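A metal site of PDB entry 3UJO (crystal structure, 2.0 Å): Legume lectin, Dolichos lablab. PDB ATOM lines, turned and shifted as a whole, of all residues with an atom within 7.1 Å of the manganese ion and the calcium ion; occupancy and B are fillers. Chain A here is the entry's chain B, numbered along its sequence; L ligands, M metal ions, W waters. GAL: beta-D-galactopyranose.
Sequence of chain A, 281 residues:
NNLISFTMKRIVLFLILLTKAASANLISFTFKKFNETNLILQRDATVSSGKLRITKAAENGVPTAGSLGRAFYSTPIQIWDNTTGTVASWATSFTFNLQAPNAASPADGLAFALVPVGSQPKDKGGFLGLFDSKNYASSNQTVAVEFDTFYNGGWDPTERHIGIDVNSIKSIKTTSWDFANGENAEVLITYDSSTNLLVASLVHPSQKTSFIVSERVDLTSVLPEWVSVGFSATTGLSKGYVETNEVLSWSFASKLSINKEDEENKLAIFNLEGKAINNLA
O of Gly 163 is in hydrogen-bond range of N of Glu 146 (2.9 Å).
Water W2 lies within hydrogen-bond range of OE1 of Glu 146, O of Ile 169 and NE1 of Trp 155. Water W4 lies within hydrogen-bond range of O of Gly 126 and NE1 of Trp 155.
Water W3 binds the calcium ion. Water W4 binds the calcium ion, 2.3 Å away. The calcium ion is bound by OD1 of Asn 152 (2.3 Å). OD2 of Asp 156 binds the calcium ion (2.4 Å). OD2 of Asp 148 binds the calcium ion (2.5 Å). The calcium ion is bound by O of Phe 150 (2.6 Å). The calcium ion is bound by OD1 of Asp 148 (2.6 Å). The calcium ion has seven donor atoms within binding distance.
The nearest printed residue that does not touch the calcium ion is Asp 108 (4.3 Å).
The nearest printed residue that does not touch the manganese ion is Ser 171 (4.2 Å).
The side-chain amide nitrogen of Asn 152 is in hydrogen-bond range of an oxygen (O3) of the ligand, at 3.1 Å. O4 of the ligand lies within hydrogen-bond range of OD2 of Asp 108 (2.6 Å). N of Gly 126 sits at hydrogen-bond distance from O3 of the ligand (2.9 Å).
Water W2 is bound to the manganese ion. OD1 of Asp 156 binds the manganese ion (2.0 Å). The manganese ion is bound by the side-chain carboxylate (OE2) of Glu 146 (2.1 Å). The manganese ion is bound by water W1 (2.2 Å). The manganese ion is bound by NE2 of His 161 (2.3 Å). The side-chain carboxylate (OD2) of Asp 148 is bound to the manganese ion, 2.4 Å away.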
ATOM      1  N   ASP A 108     -12.841   0.201  23.710  1.00  0.00           N
ATOM      2  CA  ASP A 108     -13.500  -0.356  22.526  1.00  0.00           C
ATOM      3  C   ASP A 108     -13.027  -1.767  22.169  1.00  0.00           C
ATOM      4  O   ASP A 108     -13.684  -2.448  21.373  1.00  0.00           O
ATOM      5  CB  ASP A 108     -13.300   0.567  21.321  1.00  0.00           C
ATOM      6  CG  ASP A 108     -14.438   1.550  21.140  1.00  0.00           C
ATOM      7  OD1 ASP A 108     -15.577   1.103  20.877  1.00  0.00           O
ATOM      8  OD2 ASP A 108     -14.204   2.761  21.266  1.00  0.00           O
ATOM      9  N   GLY A 109     -11.910  -2.193  22.745  1.00  0.00           N
ATOM     10  CA  GLY A 109     -11.338  -3.519  22.485  1.00  0.00           C
ATOM     11  C   GLY A 109      -9.921  -3.474  21.930  1.00  0.00           C
ATOM     12  O   GLY A 109      -9.361  -2.396  21.737  1.00  0.00           O
ATOM     13  N   GLY A 125     -11.088   4.791  18.918  1.00  0.00           N
ATOM     14  CA  GLY A 125     -12.423   4.303  19.240  1.00  0.00           C
ATOM     15  C   GLY A 125     -12.821   3.015  18.568  1.00  0.00           C
ATOM     16  O   GLY A 125     -12.094   2.022  18.614  1.00  0.00           O
ATOM     17  N   GLY A 126     -14.000   3.019  17.936  1.00  0.00           N
ATOM     18  CA  GLY A 126     -14.545   1.842  17.263  1.00  0.00           C
ATOM     19  C   GLY A 126     -13.725   1.333  16.093  1.00  0.00           C
ATOM     20  O   GLY A 126     -13.936   0.219  15.624  1.00  0.00           O
ATOM     21  N   PHE A 127     -12.786   2.157  15.635  1.00  0.00           N
ATOM     22  CA  PHE A 127     -11.881   1.785  14.552  1.00  0.00           C
ATOM     23  C   PHE A 127     -10.625   1.095  15.076  1.00  0.00           C
ATOM     24  O   PHE A 127      -9.834   0.550  14.309  1.00  0.00           O
ATOM     25  CB  PHE A 127     -11.512   3.005  13.701  1.00  0.00           C
ATOM     26  CG  PHE A 127     -12.670   3.618  12.988  1.00  0.00           C
ATOM     27  CD1 PHE A 127     -13.088   3.121  11.754  1.00  0.00           C
ATOM     28  CD2 PHE A 127     -13.357   4.685  13.549  1.00  0.00           C
ATOM     29  CE1 PHE A 127     -14.173   3.691  11.091  1.00  0.00           C
ATOM     30  CE2 PHE A 127     -14.442   5.257  12.895  1.00  0.00           C
ATOM     31  CZ  PHE A 127     -14.849   4.759  11.661  1.00  0.00           C
ATOM     32  N   LEU A 128     -10.439   1.156  16.399  1.00  0.00           N
ATOM     33  CA  LEU A 128      -9.390   0.406  17.115  1.00  0.00           C
ATOM     34  C   LEU A 128      -7.947   0.780  16.754  1.00  0.00           C
ATOM     35  O   LEU A 128      -7.014   0.040  17.051  1.00  0.00           O
ATOM     36  CB  LEU A 128      -9.624  -1.110  17.005  1.00  0.00           C
ATOM     37  CG  LEU A 128     -10.973  -1.669  17.492  1.00  0.00           C
ATOM     38  CD1 LEU A 128     -11.193  -3.093  16.999  1.00  0.00           C
ATOM     39  CD2 LEU A 128     -11.087  -1.611  19.016  1.00  0.00           C
ATOM     40  N   GLU A 146      -9.957  -8.793  15.454  1.00  0.00           N
ATOM     41  CA  GLU A 146     -10.412  -7.912  16.518  1.00  0.00           C
ATOM     42  C   GLU A 146     -11.044  -8.680  17.680  1.00  0.00           C
ATOM     43  O   GLU A 146     -11.650  -9.738  17.503  1.00  0.00           O
ATOM     44  CB  GLU A 146     -11.364  -6.833  15.986  1.00  0.00           C
ATOM     45  CG  GLU A 146     -12.695  -7.355  15.450  1.00  0.00           C
ATOM     46  CD  GLU A 146     -13.726  -6.255  15.259  1.00  0.00           C
ATOM     47  OE1 GLU A 146     -13.356  -5.142  14.834  1.00  0.00           O
ATOM     48  OE2 GLU A 146     -14.919  -6.518  15.510  1.00  0.00           O
ATOM     49  N   PHE A 147     -10.872  -8.136  18.883  1.00  0.00           N
ATOM     50  CA  PHE A 147     -11.586  -8.605  20.051  1.00  0.00           C
ATOM     51  C   PHE A 147     -12.386  -7.408  20.566  1.00  0.00           C
ATOM     52  O   PHE A 147     -11.886  -6.562  21.300  1.00  0.00           O
ATOM     53  CB  PHE A 147     -10.627  -9.194  21.083  1.00  0.00           C
ATOM     54  CG  PHE A 147      -9.835 -10.370  20.564  1.00  0.00           C
ATOM     55  CD1 PHE A 147     -10.385 -11.648  20.569  1.00  0.00           C
ATOM     56  CD2 PHE A 147      -8.555 -10.196  20.055  1.00  0.00           C
ATOM     57  CE1 PHE A 147      -9.663 -12.739  20.075  1.00  0.00           C
ATOM     58  CE2 PHE A 147      -7.832 -11.277  19.558  1.00  0.00           C
ATOM     59  CZ  PHE A 147      -8.381 -12.553  19.574  1.00  0.00           C
ATOM     60  N   ASP A 148     -13.636  -7.360  20.119  1.00  0.00           N
ATOM     61  CA  ASP A 148     -14.440  -6.153  20.175  1.00  0.00           C
ATOM     62  C   ASP A 148     -15.433  -6.207  21.335  1.00  0.00           C
ATOM     63  O   ASP A 148     -16.294  -7.075  21.385  1.00  0.00           O
ATOM     64  CB  ASP A 148     -15.192  -5.986  18.846  1.00  0.00           C
ATOM     65  CG  ASP A 148     -15.741  -4.592  18.657  1.00  0.00           C
ATOM     66  OD1 ASP A 148     -16.069  -3.913  19.658  1.00  0.00           O
ATOM     67  OD2 ASP A 148     -15.860  -4.175  17.481  1.00  0.00           O
ATOM     68  N   THR A 149     -15.298  -5.248  22.248  1.00  0.00           N
ATOM     69  CA  THR A 149     -16.163  -5.162  23.425  1.00  0.00           C
ATOM     70  C   THR A 149     -17.093  -3.940  23.416  1.00  0.00           C
ATOM     71  O   THR A 149     -17.521  -3.473  24.475  1.00  0.00           O
ATOM     72  CB  THR A 149     -15.349  -5.168  24.734  1.00  0.00           C
ATOM     73  OG1 THR A 149     -14.223  -4.300  24.595  1.00  0.00           O
ATOM     74  CG2 THR A 149     -14.876  -6.566  25.067  1.00  0.00           C
ATOM     75  N   PHE A 150     -17.390  -3.419  22.229  1.00  0.00           N
ATOM     76  CA  PHE A 150     -18.354  -2.328  22.092  1.00  0.00           C
ATOM     77  C   PHE A 150     -19.162  -2.433  20.802  1.00  0.00           C
ATOM     78  O   PHE A 150     -18.608  -2.482  19.708  1.00  0.00           O
ATOM     79  CB  PHE A 150     -17.674  -0.956  22.192  1.00  0.00           C
ATOM     80  CG  PHE A 150     -18.632   0.203  22.153  1.00  0.00           C
ATOM     81  CD1 PHE A 150     -19.001   0.782  20.946  1.00  0.00           C
ATOM     82  CD2 PHE A 150     -19.180   0.709  23.337  1.00  0.00           C
ATOM     83  CE1 PHE A 150     -19.900   1.850  20.904  1.00  0.00           C
ATOM     84  CE2 PHE A 150     -20.069   1.778  23.305  1.00  0.00           C
ATOM     85  CZ  PHE A 150     -20.428   2.353  22.088  1.00  0.00           C
ATOM     86  N   TYR A 151     -20.481  -2.449  20.966  1.00  0.00           N
ATOM     87  CA  TYR A 151     -21.421  -2.502  19.859  1.00  0.00           C
ATOM     88  C   TYR A 151     -21.505  -1.153  19.153  1.00  0.00           C
ATOM     89  O   TYR A 151     -22.146  -0.217  19.647  1.00  0.00           O
ATOM     90  CB  TYR A 151     -22.797  -2.947  20.386  1.00  0.00           C
ATOM     91  CG  TYR A 151     -23.902  -3.087  19.355  1.00  0.00           C
ATOM     92  CD1 TYR A 151     -23.686  -3.748  18.146  1.00  0.00           C
ATOM     93  CD2 TYR A 151     -25.179  -2.601  19.610  1.00  0.00           C
ATOM     94  CE1 TYR A 151     -24.703  -3.893  17.208  1.00  0.00           C
ATOM     95  CE2 TYR A 151     -26.206  -2.743  18.681  1.00  0.00           C
ATOM     96  CZ  TYR A 151     -25.969  -3.394  17.481  1.00  0.00           C
ATOM     97  OH  TYR A 151     -26.976  -3.537  16.563  1.00  0.00           O
ATOM     98  N   ASN A 152     -20.848  -1.054  17.992  1.00  0.00           N
ATOM     99  CA  ASN A 152     -20.864   0.179  17.207  1.00  0.00           C
ATOM    100  C   ASN A 152     -22.084   0.344  16.301  1.00  0.00           C
ATOM    101  O   ASN A 152     -22.452   1.456  15.941  1.00  0.00           O
ATOM    102  CB  ASN A 152     -19.568   0.315  16.390  1.00  0.00           C
ATOM    103  CG  ASN A 152     -18.433   0.944  17.200  1.00  0.00           C
ATOM    104  OD1 ASN A 152     -17.541   0.246  17.692  1.00  0.00           O
ATOM    105  ND2 ASN A 152     -18.468   2.267  17.343  1.00  0.00           N
ATOM    106  N   GLY A 153     -22.712  -0.776  15.932  1.00  0.00           N
ATOM    107  CA  GLY A 153     -23.963  -0.738  15.151  1.00  0.00           C
ATOM    108  C   GLY A 153     -23.774  -0.437  13.684  1.00  0.00           C
ATOM    109  O   GLY A 153     -24.328  -1.114  12.817  1.00  0.00           O
ATOM    110  N   TRP A 155     -21.590  -1.227  11.937  1.00  0.00           N
ATOM    111  CA  TRP A 155     -20.987  -2.403  11.335  1.00  0.00           C
ATOM    112  C   TRP A 155     -21.034  -3.623  12.260  1.00  0.00           C
ATOM    113  O   TRP A 155     -21.086  -4.758  11.787  1.00  0.00           O
ATOM    114  CB  TRP A 155     -19.541  -2.102  10.916  1.00  0.00           C
ATOM    115  CG  TRP A 155     -18.670  -1.491  11.991  1.00  0.00           C
ATOM    116  CD1 TRP A 155     -17.847  -2.164  12.854  1.00  0.00           C
ATOM    117  CD2 TRP A 155     -18.520  -0.100  12.307  1.00  0.00           C
ATOM    118  NE1 TRP A 155     -17.203  -1.269  13.682  1.00  0.00           N
ATOM    119  CE2 TRP A 155     -17.593  -0.003  13.365  1.00  0.00           C
ATOM    120  CE3 TRP A 155     -19.075   1.079  11.780  1.00  0.00           C
ATOM    121  CZ2 TRP A 155     -17.219   1.228  13.925  1.00  0.00           C
ATOM    122  CZ3 TRP A 155     -18.703   2.300  12.342  1.00  0.00           C
ATOM    123  CH2 TRP A 155     -17.780   2.367  13.396  1.00  0.00           C
ATOM    124  N   ASP A 156     -21.056  -3.381  13.568  1.00  0.00           N
ATOM    125  CA  ASP A 156     -20.956  -4.455  14.559  1.00  0.00           C
ATOM    126  C   ASP A 156     -22.188  -5.358  14.703  1.00  0.00           C
ATOM    127  O   ASP A 156     -23.323  -4.894  14.547  1.00  0.00           O
ATOM    128  CB  ASP A 156     -20.594  -3.885  15.932  1.00  0.00           C
ATOM    129  CG  ASP A 156     -19.097  -3.659  16.097  1.00  0.00           C
ATOM    130  OD1 ASP A 156     -18.310  -4.309  15.369  1.00  0.00           O
ATOM    131  OD2 ASP A 156     -18.708  -2.855  16.969  1.00  0.00           O
ATOM    132  N   PRO A 157     -21.962  -6.649  14.993  1.00  0.00           N
ATOM    133  CA  PRO A 157     -23.011  -7.531  15.502  1.00  0.00           C
ATOM    134  C   PRO A 157     -23.382  -7.146  16.943  1.00  0.00           C
ATOM    135  O   PRO A 157     -22.623  -6.424  17.590  1.00  0.00           O
ATOM    136  CB  PRO A 157     -22.365  -8.926  15.479  1.00  0.00           C
ATOM    137  CG  PRO A 157     -21.218  -8.804  14.531  1.00  0.00           C
ATOM    138  CD  PRO A 157     -20.728  -7.406  14.686  1.00  0.00           C
ATOM    139  N   HIS A 161     -17.671  -9.584  20.491  1.00  0.00           N
ATOM    140  CA  HIS A 161     -17.340 -10.432  19.349  1.00  0.00           C
ATOM    141  C   HIS A 161     -15.882 -10.423  18.913  1.00  0.00           C
ATOM    142  O   HIS A 161     -15.156  -9.449  19.116  1.00  0.00           O
ATOM    143  CB  HIS A 161     -18.234 -10.077  18.157  1.00  0.00           C
ATOM    144  CG  HIS A 161     -18.115  -8.659  17.694  1.00  0.00           C
ATOM    145  ND1 HIS A 161     -18.807  -7.626  18.292  1.00  0.00           N
ATOM    146  CD2 HIS A 161     -17.393  -8.099  16.693  1.00  0.00           C
ATOM    147  CE1 HIS A 161     -18.509  -6.496  17.680  1.00  0.00           C
ATOM    148  NE2 HIS A 161     -17.653  -6.758  16.709  1.00  0.00           N
ATOM    149  N   ILE A 162     -15.474 -11.547  18.340  1.00  0.00           N
ATOM    150  CA  ILE A 162     -14.215 -11.665  17.620  1.00  0.00           C
ATOM    151  C   ILE A 162     -14.549 -11.499  16.143  1.00  0.00           C
ATOM    152  O   ILE A 162     -15.544 -12.056  15.667  1.00  0.00           O
ATOM    153  CB  ILE A 162     -13.534 -13.034  17.878  1.00  0.00           C
ATOM    154  CG1 ILE A 162     -13.451 -13.335  19.377  1.00  0.00           C
ATOM    155  CG2 ILE A 162     -12.136 -13.072  17.246  1.00  0.00           C
ATOM    156  CD1 ILE A 162     -13.072 -14.760  19.724  1.00  0.00           C
ATOM    157  N   GLY A 163     -13.747 -10.711  15.436  1.00  0.00           N
ATOM    158  CA  GLY A 163     -13.971 -10.470  14.007  1.00  0.00           C
ATOM    159  C   GLY A 163     -12.706 -10.567  13.182  1.00  0.00           C
ATOM    160  O   GLY A 163     -11.600 -10.321  13.666  1.00  0.00           O
ATOM    161  N   ASP A 165     -10.928  -8.760  10.131  1.00  0.00           N
ATOM    162  CA  ASP A 165     -10.979  -7.458   9.475  1.00  0.00           C
ATOM    163  C   ASP A 165     -10.032  -7.382   8.290  1.00  0.00           C
ATOM    164  O   ASP A 165      -8.810  -7.488   8.453  1.00  0.00           O
ATOM    165  CB  ASP A 165     -10.654  -6.336  10.472  1.00  0.00           C
ATOM    166  CG  ASP A 165     -11.684  -6.219  11.580  1.00  0.00           C
ATOM    167  OD1 ASP A 165     -12.570  -7.103  11.694  1.00  0.00           O
ATOM    168  OD2 ASP A 165     -11.613  -5.246  12.358  1.00  0.00           O
ATOM    169  N   ILE A 169     -13.198  -1.906   9.016  1.00  0.00           N
ATOM    170  CA  ILE A 169     -13.632  -2.181  10.394  1.00  0.00           C
ATOM    171  C   ILE A 169     -14.946  -2.974  10.406  1.00  0.00           C
ATOM    172  O   ILE A 169     -15.331  -3.578  11.418  1.00  0.00           O
ATOM    173  CB  ILE A 169     -13.721  -0.866  11.240  1.00  0.00           C
ATOM    174  CG1 ILE A 169     -13.860  -1.168  12.738  1.00  0.00           C
ATOM    175  CG2 ILE A 169     -14.857   0.048  10.736  1.00  0.00           C
ATOM    176  CD1 ILE A 169     -12.619  -1.788  13.361  1.00  0.00           C
ATOM    177  N   LYS A 170     -15.626  -2.977   9.262  1.00  0.00           N
ATOM    178  CA  LYS A 170     -16.762  -3.864   9.008  1.00  0.00           C
ATOM    179  C   LYS A 170     -16.218  -5.258   8.740  1.00  0.00           C
ATOM    180  O   LYS A 170     -15.704  -5.536   7.656  1.00  0.00           O
ATOM    181  CB  LYS A 170     -17.563  -3.346   7.817  1.00  0.00           C
ATOM    182  CG  LYS A 170     -18.965  -3.923   7.657  1.00  0.00           C
ATOM    183  CD  LYS A 170     -19.825  -2.980   6.845  1.00  0.00           C
ATOM    184  CE  LYS A 170     -21.182  -3.575   6.505  1.00  0.00           C
ATOM    185  NZ  LYS A 170     -22.078  -2.546   5.912  1.00  0.00           N
ATOM    186  N   SER A 171     -16.345  -6.137   9.733  1.00  0.00           N
ATOM    187  CA  SER A 171     -15.772  -7.484   9.691  1.00  0.00           C
ATOM    188  C   SER A 171     -16.375  -8.362   8.586  1.00  0.00           C
ATOM    189  O   SER A 171     -17.582  -8.326   8.335  1.00  0.00           O
ATOM    190  CB  SER A 171     -15.917  -8.181  11.048  1.00  0.00           C
ATOM    191  OG  SER A 171     -15.300  -7.439  12.087  1.00  0.00           O
ATOM    192  N   THR A 174     -17.704 -12.809  11.780  1.00  0.00           N
ATOM    193  CA  THR A 174     -17.705 -12.606  13.227  1.00  0.00           C
ATOM    194  C   THR A 174     -18.155 -13.871  13.943  1.00  0.00           C
ATOM    195  O   THR A 174     -18.765 -14.758  13.348  1.00  0.00           O
ATOM    196  CB  THR A 174     -18.625 -11.431  13.644  1.00  0.00           C
ATOM    197  OG1 THR A 174     -19.879 -11.550  12.953  1.00  0.00           O
ATOM    198  CG2 THR A 174     -17.995 -10.092  13.302  1.00  0.00           C
HETATM  199  C1  GAL L   1     -18.336   6.573  20.244  1.00  0.00           C
HETATM  200  C2  GAL L   1     -17.397   5.673  19.442  1.00  0.00           C
HETATM  201  C3  GAL L   1     -17.389   4.265  20.046  1.00  0.00           C
HETATM  202  C4  GAL L   1     -17.096   4.333  21.541  1.00  0.00           C
HETATM  203  C5  GAL L   1     -18.097   5.261  22.226  1.00  0.00           C
HETATM  204  C6  GAL L   1     -17.818   5.383  23.721  1.00  0.00           C
HETATM  205  O1  GAL L   1     -18.160   7.895  19.810  1.00  0.00           O
HETATM  206  O2  GAL L   1     -17.783   5.622  18.085  1.00  0.00           O
HETATM  207  O3  GAL L   1     -16.433   3.464  19.409  1.00  0.00           O
HETATM  208  O4  GAL L   1     -15.777   4.824  21.727  1.00  0.00           O
HETATM  209  O5  GAL L   1     -18.033   6.538  21.626  1.00  0.00           O
HETATM  210  O6  GAL L   1     -18.974   5.815  24.384  1.00  0.00           O
HETATM  211 MN    MN M   1     -16.522  -5.211  15.408  1.00  0.00          MN
HETATM  212 CA    CA M   2     -16.744  -1.907  18.064  1.00  0.00          CA
HETATM  213  O   HOH W   1     -17.211  -6.513  13.719  1.00  0.00           O
HETATM  214  O   HOH W   2     -15.545  -4.026  14.315  1.00  0.00           O
HETATM  215  O   HOH W   3     -15.391  -1.269  19.646  1.00  0.00           O
HETATM  216  O   HOH W   4     -15.717  -1.508  16.017  1.00  0.00           O
